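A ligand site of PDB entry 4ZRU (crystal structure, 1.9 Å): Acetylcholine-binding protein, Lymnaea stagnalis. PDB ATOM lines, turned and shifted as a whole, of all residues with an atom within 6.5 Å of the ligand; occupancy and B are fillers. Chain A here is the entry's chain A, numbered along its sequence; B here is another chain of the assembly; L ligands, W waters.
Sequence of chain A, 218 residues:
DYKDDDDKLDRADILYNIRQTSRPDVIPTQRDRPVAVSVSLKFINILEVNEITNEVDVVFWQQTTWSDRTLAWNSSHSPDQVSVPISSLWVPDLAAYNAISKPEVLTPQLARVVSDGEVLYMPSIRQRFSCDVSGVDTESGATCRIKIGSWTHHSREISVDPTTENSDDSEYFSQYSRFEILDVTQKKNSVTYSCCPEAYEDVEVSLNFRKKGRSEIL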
ATOM      1  N   TYR A  97       1.036   9.401 -26.060  1.00  0.00           N
ATOM      2  CA  TYR A  97       1.443   9.238 -24.667  1.00  0.00           C
ATOM      3  C   TYR A  97       0.672  10.120 -23.700  1.00  0.00           C
ATOM      4  O   TYR A  97       0.557   9.786 -22.517  1.00  0.00           O
ATOM      5  CB  TYR A  97       2.941   9.538 -24.529  1.00  0.00           C
ATOM      6  CG  TYR A  97       3.807   8.403 -24.977  1.00  0.00           C
ATOM      7  CD1 TYR A  97       4.061   8.171 -26.324  1.00  0.00           C
ATOM      8  CD2 TYR A  97       4.365   7.541 -24.048  1.00  0.00           C
ATOM      9  CE1 TYR A  97       4.875   7.103 -26.727  1.00  0.00           C
ATOM     10  CE2 TYR A  97       5.153   6.489 -24.433  1.00  0.00           C
ATOM     11  CZ  TYR A  97       5.404   6.267 -25.761  1.00  0.00           C
ATOM     12  OH  TYR A  97       6.215   5.187 -26.097  1.00  0.00           O
ATOM     13  N   SER A 150       4.855   4.210 -31.427  1.00  0.00           N
ATOM     14  CA  SER A 150       4.470   2.825 -31.235  1.00  0.00           C
ATOM     15  C   SER A 150       4.362   2.540 -29.752  1.00  0.00           C
ATOM     16  O   SER A 150       5.280   2.857 -28.973  1.00  0.00           O
ATOM     17  CB  SER A 150       5.477   1.875 -31.892  1.00  0.00           C
ATOM     18  OG  SER A 150       5.204   0.520 -31.539  1.00  0.00           O
ATOM     19  N   TRP A 151       3.247   1.945 -29.351  1.00  0.00           N
ATOM     20  CA  TRP A 151       3.081   1.573 -27.947  1.00  0.00           C
ATOM     21  C   TRP A 151       3.998   0.422 -27.536  1.00  0.00           C
ATOM     22  O   TRP A 151       4.552   0.415 -26.434  1.00  0.00           O
ATOM     23  CB  TRP A 151       1.625   1.199 -27.655  1.00  0.00           C
ATOM     24  CG  TRP A 151       1.376   1.116 -26.173  1.00  0.00           C
ATOM     25  CD1 TRP A 151       1.071  -0.004 -25.459  1.00  0.00           C
ATOM     26  CD2 TRP A 151       1.422   2.200 -25.249  1.00  0.00           C
ATOM     27  NE1 TRP A 151       0.924   0.317 -24.117  1.00  0.00           N
ATOM     28  CE2 TRP A 151       1.135   1.666 -23.969  1.00  0.00           C
ATOM     29  CE3 TRP A 151       1.669   3.566 -25.368  1.00  0.00           C
ATOM     30  CZ2 TRP A 151       1.097   2.459 -22.823  1.00  0.00           C
ATOM     31  CZ3 TRP A 151       1.633   4.350 -24.228  1.00  0.00           C
ATOM     32  CH2 TRP A 151       1.354   3.793 -22.965  1.00  0.00           C
ATOM     33  N   THR A 152       4.169  -0.578 -28.400  1.00  0.00           N
ATOM     34  CA  THR A 152       4.873  -1.786 -27.983  1.00  0.00           C
ATOM     35  C   THR A 152       6.136  -2.125 -28.757  1.00  0.00           C
ATOM     36  O   THR A 152       6.859  -3.045 -28.376  1.00  0.00           O
ATOM     37  CB  THR A 152       3.945  -3.030 -28.047  1.00  0.00           C
ATOM     38  OG1 THR A 152       3.717  -3.401 -29.422  1.00  0.00           O
ATOM     39  CG2 THR A 152       2.610  -2.767 -27.341  1.00  0.00           C
ATOM     40  N   HIS A 153       6.423  -1.410 -29.831  1.00  0.00           N
ATOM     41  CA  HIS A 153       7.609  -1.709 -30.620  1.00  0.00           C
ATOM     42  C   HIS A 153       8.702  -0.684 -30.364  1.00  0.00           C
ATOM     43  O   HIS A 153       8.498   0.503 -30.582  1.00  0.00           O
ATOM     44  CB  HIS A 153       7.278  -1.757 -32.111  1.00  0.00           C
ATOM     45  CG  HIS A 153       6.335  -2.866 -32.486  1.00  0.00           C
ATOM     46  ND1 HIS A 153       6.752  -4.169 -32.647  1.00  0.00           N
ATOM     47  CD2 HIS A 153       5.004  -2.861 -32.761  1.00  0.00           C
ATOM     48  CE1 HIS A 153       5.723  -4.924 -32.999  1.00  0.00           C
ATOM     49  NE2 HIS A 153       4.650  -4.150 -33.066  1.00  0.00           N
ATOM     50  N   VAL A 191      11.639   8.364 -26.200  1.00  0.00           N
ATOM     51  CA  VAL A 191      11.325   8.279 -24.776  1.00  0.00           C
ATOM     52  C   VAL A 191      11.756   6.924 -24.238  1.00  0.00           C
ATOM     53  O   VAL A 191      11.835   5.934 -24.961  1.00  0.00           O
ATOM     54  CB  VAL A 191       9.825   8.482 -24.471  1.00  0.00           C
ATOM     55  CG1 VAL A 191       9.346   9.826 -24.979  1.00  0.00           C
ATOM     56  CG2 VAL A 191       9.005   7.354 -25.064  1.00  0.00           C
ATOM     57  N   THR A 192      12.045   6.914 -22.946  1.00  0.00           N
ATOM     58  CA  THR A 192      12.331   5.664 -22.264  1.00  0.00           C
ATOM     59  C   THR A 192      11.913   5.830 -20.807  1.00  0.00           C
ATOM     60  O   THR A 192      12.028   6.916 -20.255  1.00  0.00           O
ATOM     61  CB  THR A 192      13.818   5.267 -22.399  1.00  0.00           C
ATOM     62  OG1 THR A 192      14.039   3.978 -21.811  1.00  0.00           O
ATOM     63  CG2 THR A 192      14.720   6.313 -21.748  1.00  0.00           C
ATOM     64  N   TYR A 193      11.371   4.774 -20.222  1.00  0.00           N
ATOM     65  CA  TYR A 193      10.883   4.793 -18.856  1.00  0.00           C
ATOM     66  C   TYR A 193      11.485   3.615 -18.123  1.00  0.00           C
ATOM     67  O   TYR A 193      11.882   2.631 -18.741  1.00  0.00           O
ATOM     68  CB  TYR A 193       9.355   4.700 -18.801  1.00  0.00           C
ATOM     69  CG  TYR A 193       8.627   5.855 -19.467  1.00  0.00           C
ATOM     70  CD1 TYR A 193       8.403   5.850 -20.834  1.00  0.00           C
ATOM     71  CD2 TYR A 193       8.141   6.931 -18.716  1.00  0.00           C
ATOM     72  CE1 TYR A 193       7.738   6.884 -21.450  1.00  0.00           C
ATOM     73  CE2 TYR A 193       7.460   7.983 -19.327  1.00  0.00           C
ATOM     74  CZ  TYR A 193       7.269   7.943 -20.702  1.00  0.00           C
ATOM     75  OH  TYR A 193       6.595   8.969 -21.345  1.00  0.00           O
ATOM     76  N   CYS A 195      10.011   1.436 -16.454  1.00  0.00           N
ATOM     77  CA  CYS A 195       9.158   0.267 -16.660  1.00  0.00           C
ATOM     78  C   CYS A 195       9.663  -0.541 -17.853  1.00  0.00           C
ATOM     79  O   CYS A 195       9.530  -1.765 -17.914  1.00  0.00           O
ATOM     80  CB  CYS A 195       7.719   0.694 -16.910  1.00  0.00           C
ATOM     81  SG  CYS A 195       7.472   1.355 -18.580  1.00  0.00           S
ATOM     82  N   CYS A 196      10.240   0.173 -18.807  1.00  0.00           N
ATOM     83  CA  CYS A 196      10.441  -0.343 -20.157  1.00  0.00           C
ATOM     84  C   CYS A 196      11.781   0.127 -20.711  1.00  0.00           C
ATOM     85  O   CYS A 196      11.873   1.204 -21.300  1.00  0.00           O
ATOM     86  CB  CYS A 196       9.305   0.108 -21.059  1.00  0.00           C
ATOM     87  SG  CYS A 196       7.666   0.094 -20.223  1.00  0.00           S
ATOM     88  N   GLU A 198      13.867  -0.327 -23.174  1.00  0.00           N
ATOM     89  CA  GLU A 198      14.284  -0.037 -24.538  1.00  0.00           C
ATOM     90  C   GLU A 198      13.984   1.428 -24.842  1.00  0.00           C
ATOM     91  O   GLU A 198      13.308   2.098 -24.051  1.00  0.00           O
ATOM     92  CB  GLU A 198      13.558  -0.953 -25.518  1.00  0.00           C
ATOM     93  CG  GLU A 198      13.523  -2.410 -25.084  1.00  0.00           C
ATOM     94  CD  GLU A 198      14.666  -3.224 -25.662  1.00  0.00           C
ATOM     95  OE1 GLU A 198      15.499  -2.646 -26.381  1.00  0.00           O
ATOM     96  OE2 GLU A 198      14.716  -4.449 -25.405  1.00  0.00           O
ATOM     97  N   TYR A 200      12.014   4.097 -27.287  1.00  0.00           N
ATOM     98  CA  TYR A 200      10.865   4.143 -28.183  1.00  0.00           C
ATOM     99  C   TYR A 200      10.850   5.453 -28.958  1.00  0.00           C
ATOM    100  O   TYR A 200      10.965   6.512 -28.350  1.00  0.00           O
ATOM    101  CB  TYR A 200       9.560   3.979 -27.387  1.00  0.00           C
ATOM    102  CG  TYR A 200       9.466   2.628 -26.758  1.00  0.00           C
ATOM    103  CD1 TYR A 200      10.151   2.332 -25.575  1.00  0.00           C
ATOM    104  CD2 TYR A 200       8.733   1.619 -27.356  1.00  0.00           C
ATOM    105  CE1 TYR A 200      10.076   1.077 -24.998  1.00  0.00           C
ATOM    106  CE2 TYR A 200       8.660   0.354 -26.799  1.00  0.00           C
ATOM    107  CZ  TYR A 200       9.334   0.092 -25.614  1.00  0.00           C
ATOM    108  OH  TYR A 200       9.257  -1.160 -25.060  1.00  0.00           O
ATOM    109  N   TRP B  61      -1.015   3.582 -16.343  1.00  0.00           N
ATOM    110  CA  TRP B  61      -0.495   2.435 -17.088  1.00  0.00           C
ATOM    111  C   TRP B  61      -0.487   1.263 -16.123  1.00  0.00           C
ATOM    112  O   TRP B  61       0.031   1.364 -15.026  1.00  0.00           O
ATOM    113  CB  TRP B  61       0.906   2.691 -17.640  1.00  0.00           C
ATOM    114  CG  TRP B  61       1.007   3.857 -18.553  1.00  0.00           C
ATOM    115  CD1 TRP B  61      -0.017   4.588 -19.078  1.00  0.00           C
ATOM    116  CD2 TRP B  61       2.216   4.440 -19.072  1.00  0.00           C
ATOM    117  NE1 TRP B  61       0.471   5.587 -19.883  1.00  0.00           N
ATOM    118  CE2 TRP B  61       1.847   5.509 -19.889  1.00  0.00           C
ATOM    119  CE3 TRP B  61       3.574   4.152 -18.905  1.00  0.00           C
ATOM    120  CZ2 TRP B  61       2.776   6.313 -20.545  1.00  0.00           C
ATOM    121  CZ3 TRP B  61       4.507   4.943 -19.558  1.00  0.00           C
ATOM    122  CH2 TRP B  61       4.108   6.010 -20.369  1.00  0.00           C
ATOM    123  N   GLN B  81      11.728 -11.144 -28.652  1.00  0.00           N
ATOM    124  CA  GLN B  81      10.366 -10.745 -28.279  1.00  0.00           C
ATOM    125  C   GLN B  81       9.552 -10.449 -29.514  1.00  0.00           C
ATOM    126  O   GLN B  81      10.108 -10.029 -30.547  1.00  0.00           O
ATOM    127  CB  GLN B  81      10.357  -9.470 -27.410  1.00  0.00           C
ATOM    128  CG  GLN B  81      11.170  -9.477 -26.167  1.00  0.00           C
ATOM    129  CD  GLN B  81      10.882  -8.253 -25.309  1.00  0.00           C
ATOM    130  OE1 GLN B  81       9.899  -7.517 -25.548  1.00  0.00           O
ATOM    131  NE2 GLN B  81      11.709  -8.017 -24.302  1.00  0.00           N
ATOM    132  N   LEU B 110      -2.134  -4.942 -27.466  1.00  0.00           N
ATOM    133  CA  LEU B 110      -1.037  -5.862 -27.746  1.00  0.00           C
ATOM    134  C   LEU B 110      -0.200  -6.099 -26.477  1.00  0.00           C
ATOM    135  O   LEU B 110       0.031  -5.174 -25.694  1.00  0.00           O
ATOM    136  CB  LEU B 110      -0.129  -5.303 -28.840  1.00  0.00           C
ATOM    137  CG  LEU B 110      -0.744  -4.921 -30.181  1.00  0.00           C
ATOM    138  CD1 LEU B 110       0.324  -4.312 -31.088  1.00  0.00           C
ATOM    139  CD2 LEU B 110      -1.373  -6.156 -30.845  1.00  0.00           C
ATOM    140  N   ALA B 111       0.261  -7.336 -26.311  1.00  0.00           N
ATOM    141  CA  ALA B 111       1.237  -7.668 -25.289  1.00  0.00           C
ATOM    142  C   ALA B 111       2.586  -8.031 -25.942  1.00  0.00           C
ATOM    143  O   ALA B 111       2.645  -8.324 -27.132  1.00  0.00           O
ATOM    144  CB  ALA B 111       0.721  -8.833 -24.427  1.00  0.00           C
ATOM    145  N   ARG B 112       3.658  -8.018 -25.158  1.00  0.00           N
ATOM    146  CA  ARG B 112       4.926  -8.554 -25.610  1.00  0.00           C
ATOM    147  C   ARG B 112       5.078  -9.990 -25.076  1.00  0.00           C
ATOM    148  O   ARG B 112       4.806 -10.235 -23.904  1.00  0.00           O
ATOM    149  CB  ARG B 112       6.085  -7.667 -25.106  1.00  0.00           C
ATOM    150  CG  ARG B 112       6.135  -6.285 -25.777  1.00  0.00           C
ATOM    151  CD  ARG B 112       6.454  -6.443 -27.251  1.00  0.00           C
ATOM    152  NE  ARG B 112       7.889  -6.501 -27.468  1.00  0.00           N
ATOM    153  CZ  ARG B 112       8.483  -6.275 -28.639  1.00  0.00           C
ATOM    154  NH1 ARG B 112       7.750  -6.013 -29.709  1.00  0.00           N
ATOM    155  NH2 ARG B 112       9.825  -6.327 -28.729  1.00  0.00           N
ATOM    156  N   LEU B 120       4.274  -9.605 -21.216  1.00  0.00           N
ATOM    157  CA  LEU B 120       4.254  -8.245 -20.693  1.00  0.00           C
ATOM    158  C   LEU B 120       3.110  -7.486 -21.340  1.00  0.00           C
ATOM    159  O   LEU B 120       3.081  -7.328 -22.553  1.00  0.00           O
ATOM    160  CB  LEU B 120       5.573  -7.521 -20.976  1.00  0.00           C
ATOM    161  CG  LEU B 120       6.840  -8.385 -21.019  1.00  0.00           C
ATOM    162  CD1 LEU B 120       7.963  -7.637 -21.762  1.00  0.00           C
ATOM    163  CD2 LEU B 120       7.275  -8.725 -19.603  1.00  0.00           C
ATOM    164  N   TYR B 121       2.183  -7.010 -20.527  1.00  0.00           N
ATOM    165  CA  TYR B 121       1.013  -6.284 -21.055  1.00  0.00           C
ATOM    166  C   TYR B 121       0.858  -5.021 -20.229  1.00  0.00           C
ATOM    167  O   TYR B 121       0.781  -5.081 -18.986  1.00  0.00           O
ATOM    168  CB  TYR B 121      -0.231  -7.166 -20.994  1.00  0.00           C
ATOM    169  CG  TYR B 121      -1.523  -6.475 -21.402  1.00  0.00           C
ATOM    170  CD1 TYR B 121      -1.612  -5.785 -22.615  1.00  0.00           C
ATOM    171  CD2 TYR B 121      -2.654  -6.524 -20.587  1.00  0.00           C
ATOM    172  CE1 TYR B 121      -2.820  -5.151 -22.998  1.00  0.00           C
ATOM    173  CE2 TYR B 121      -3.836  -5.902 -20.960  1.00  0.00           C
ATOM    174  CZ  TYR B 121      -3.910  -5.225 -22.149  1.00  0.00           C
ATOM    175  OH  TYR B 121      -5.100  -4.607 -22.485  1.00  0.00           O
ATOM    176  N   MET B 122       0.829  -3.879 -20.903  1.00  0.00           N
ATOM    177  CA  MET B 122       0.747  -2.622 -20.162  1.00  0.00           C
ATOM    178  C   MET B 122      -0.179  -1.607 -20.857  1.00  0.00           C
ATOM    179  O   MET B 122       0.283  -0.668 -21.523  1.00  0.00           O
ATOM    180  CB  MET B 122       2.149  -2.025 -19.962  1.00  0.00           C
ATOM    181  CG  MET B 122       2.160  -0.776 -19.067  1.00  0.00           C
ATOM    182  SD  MET B 122       3.807  -0.021 -18.826  1.00  0.00           S
ATOM    183  CE  MET B 122       4.018   0.827 -20.406  1.00  0.00           C
ATOM    184  N   PRO B 123      -1.493  -1.791 -20.697  1.00  0.00           N
ATOM    185  CA  PRO B 123      -2.471  -0.851 -21.244  1.00  0.00           C
ATOM    186  C   PRO B 123      -2.476   0.460 -20.475  1.00  0.00           C
ATOM    187  O   PRO B 123      -2.221   0.477 -19.267  1.00  0.00           O
ATOM    188  CB  PRO B 123      -3.789  -1.592 -21.058  1.00  0.00           C
ATOM    189  CG  PRO B 123      -3.565  -2.463 -19.840  1.00  0.00           C
ATOM    190  CD  PRO B 123      -2.119  -2.887 -19.920  1.00  0.00           C
HETATM  191  C1  LIG L   1       7.108   2.947 -23.272  1.00  0.00           C
HETATM  192  C2  LIG L   1       5.750   3.141 -22.654  1.00  0.00           C
HETATM  193  C3  LIG L   1       4.823   3.157 -23.800  1.00  0.00           C
HETATM  194  N1  LIG L   1       5.526   2.614 -24.942  1.00  0.00           N
HETATM  195  C4  LIG L   1       6.744   2.094 -24.414  1.00  0.00           C
HETATM  196  C5  LIG L   1       6.458   0.691 -24.002  1.00  0.00           C
HETATM  197  C6  LIG L   1       6.078  -0.413 -23.737  1.00  0.00           C
HETATM  198  C7  LIG L   1       5.494  -1.766 -23.496  1.00  0.00           C
HETATM  199  C8  LIG L   1       6.256  -2.827 -23.047  1.00  0.00           C
HETATM  200  C9  LIG L   1       5.604  -4.046 -22.860  1.00  0.00           C
HETATM  201  C10 LIG L   1       4.160  -1.906 -23.732  1.00  0.00           C
HETATM  202  N2  LIG L   1       3.582  -3.060 -23.533  1.00  0.00           N
HETATM  203  C11 LIG L   1       4.271  -4.127 -23.105  1.00  0.00           C
HETATM  204  O   HOH W   1       0.844  -3.453 -23.777  1.00  0.00           O
HETATM  205  O   HOH W   2       5.631  -3.056 -19.565  1.00  0.00           O
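The indole nitrogen of Trp 151 sits at hydrogen-bond distance from the backbone carbonyl oxygen of Met 122 of chain B, at 2.8 Å.
O of Tyr 200 sits at hydrogen-bond distance from N of Val 191 (2.9 Å).
The backbone carbonyl oxygen (O) of Leu 120 of chain B lies within hydrogen-bond range of the backbone NH (N) of Arg 112 of chain B (2.8 Å).
O of Thr 152 lies within hydrogen-bond range of NH1 of Arg 112 of chain B, at 3.4 Å.
The side-chain amide oxygen (OE1) of Gln 81 of chain B is in hydrogen-bond range of the guanidinium group (NE) of Arg 112 of chain B (3.0 Å).
SG of Cys 196 is disulfide-bonded to SG of Cys 195.
The side-chain hydroxyl (OG) of Ser 150 lies close to the backbone NH (N) of Thr 152, at 3.5 Å.
The backbone carbonyl oxygen (O) of Trp 151 is in hydrogen-bond range of a nitrogen (N1) of the ligand, 2.8 Å away.
The side-chain hydroxyl (OH) of Tyr 97 lies within hydrogen-bond range of a nitrogen (N1) of the ligand.
CG2 of Thr 152 touches N2 of the ligand, 3.9 Å away.
Cys 196 touches the ligand.
Tyr 200 touches the ligand.
CZ3 of Trp 61 of chain B touches C2 of the ligand, 3.8 Å away.
Arg 112 of chain B touches the ligand (CG to C9, 3.7 Å).
O of Leu 120 of chain B touches C11 of the ligand (3.5 Å).
CE of Met 122 of chain B touches C2 of the ligand, 3.7 Å away.
Within 4 Å of the ligand: Tyr 97, Trp 151, Thr 152, Cys 196, Tyr 200, Trp 61 of chain B, Arg 112 of chain B, Leu 120 of chain B and Met 122 of chain B.
The nearest printed residue that does not touch the ligand is Tyr 193 (4.01 Å).
Water W1 lies within hydrogen-bond range of the backbone carbonyl oxygen of Leu 110 of chain B (2.7 Å), a nitrogen (N2) of the ligand (2.8 Å) and the backbone NH of Met 122 of chain B (2.9 Å).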
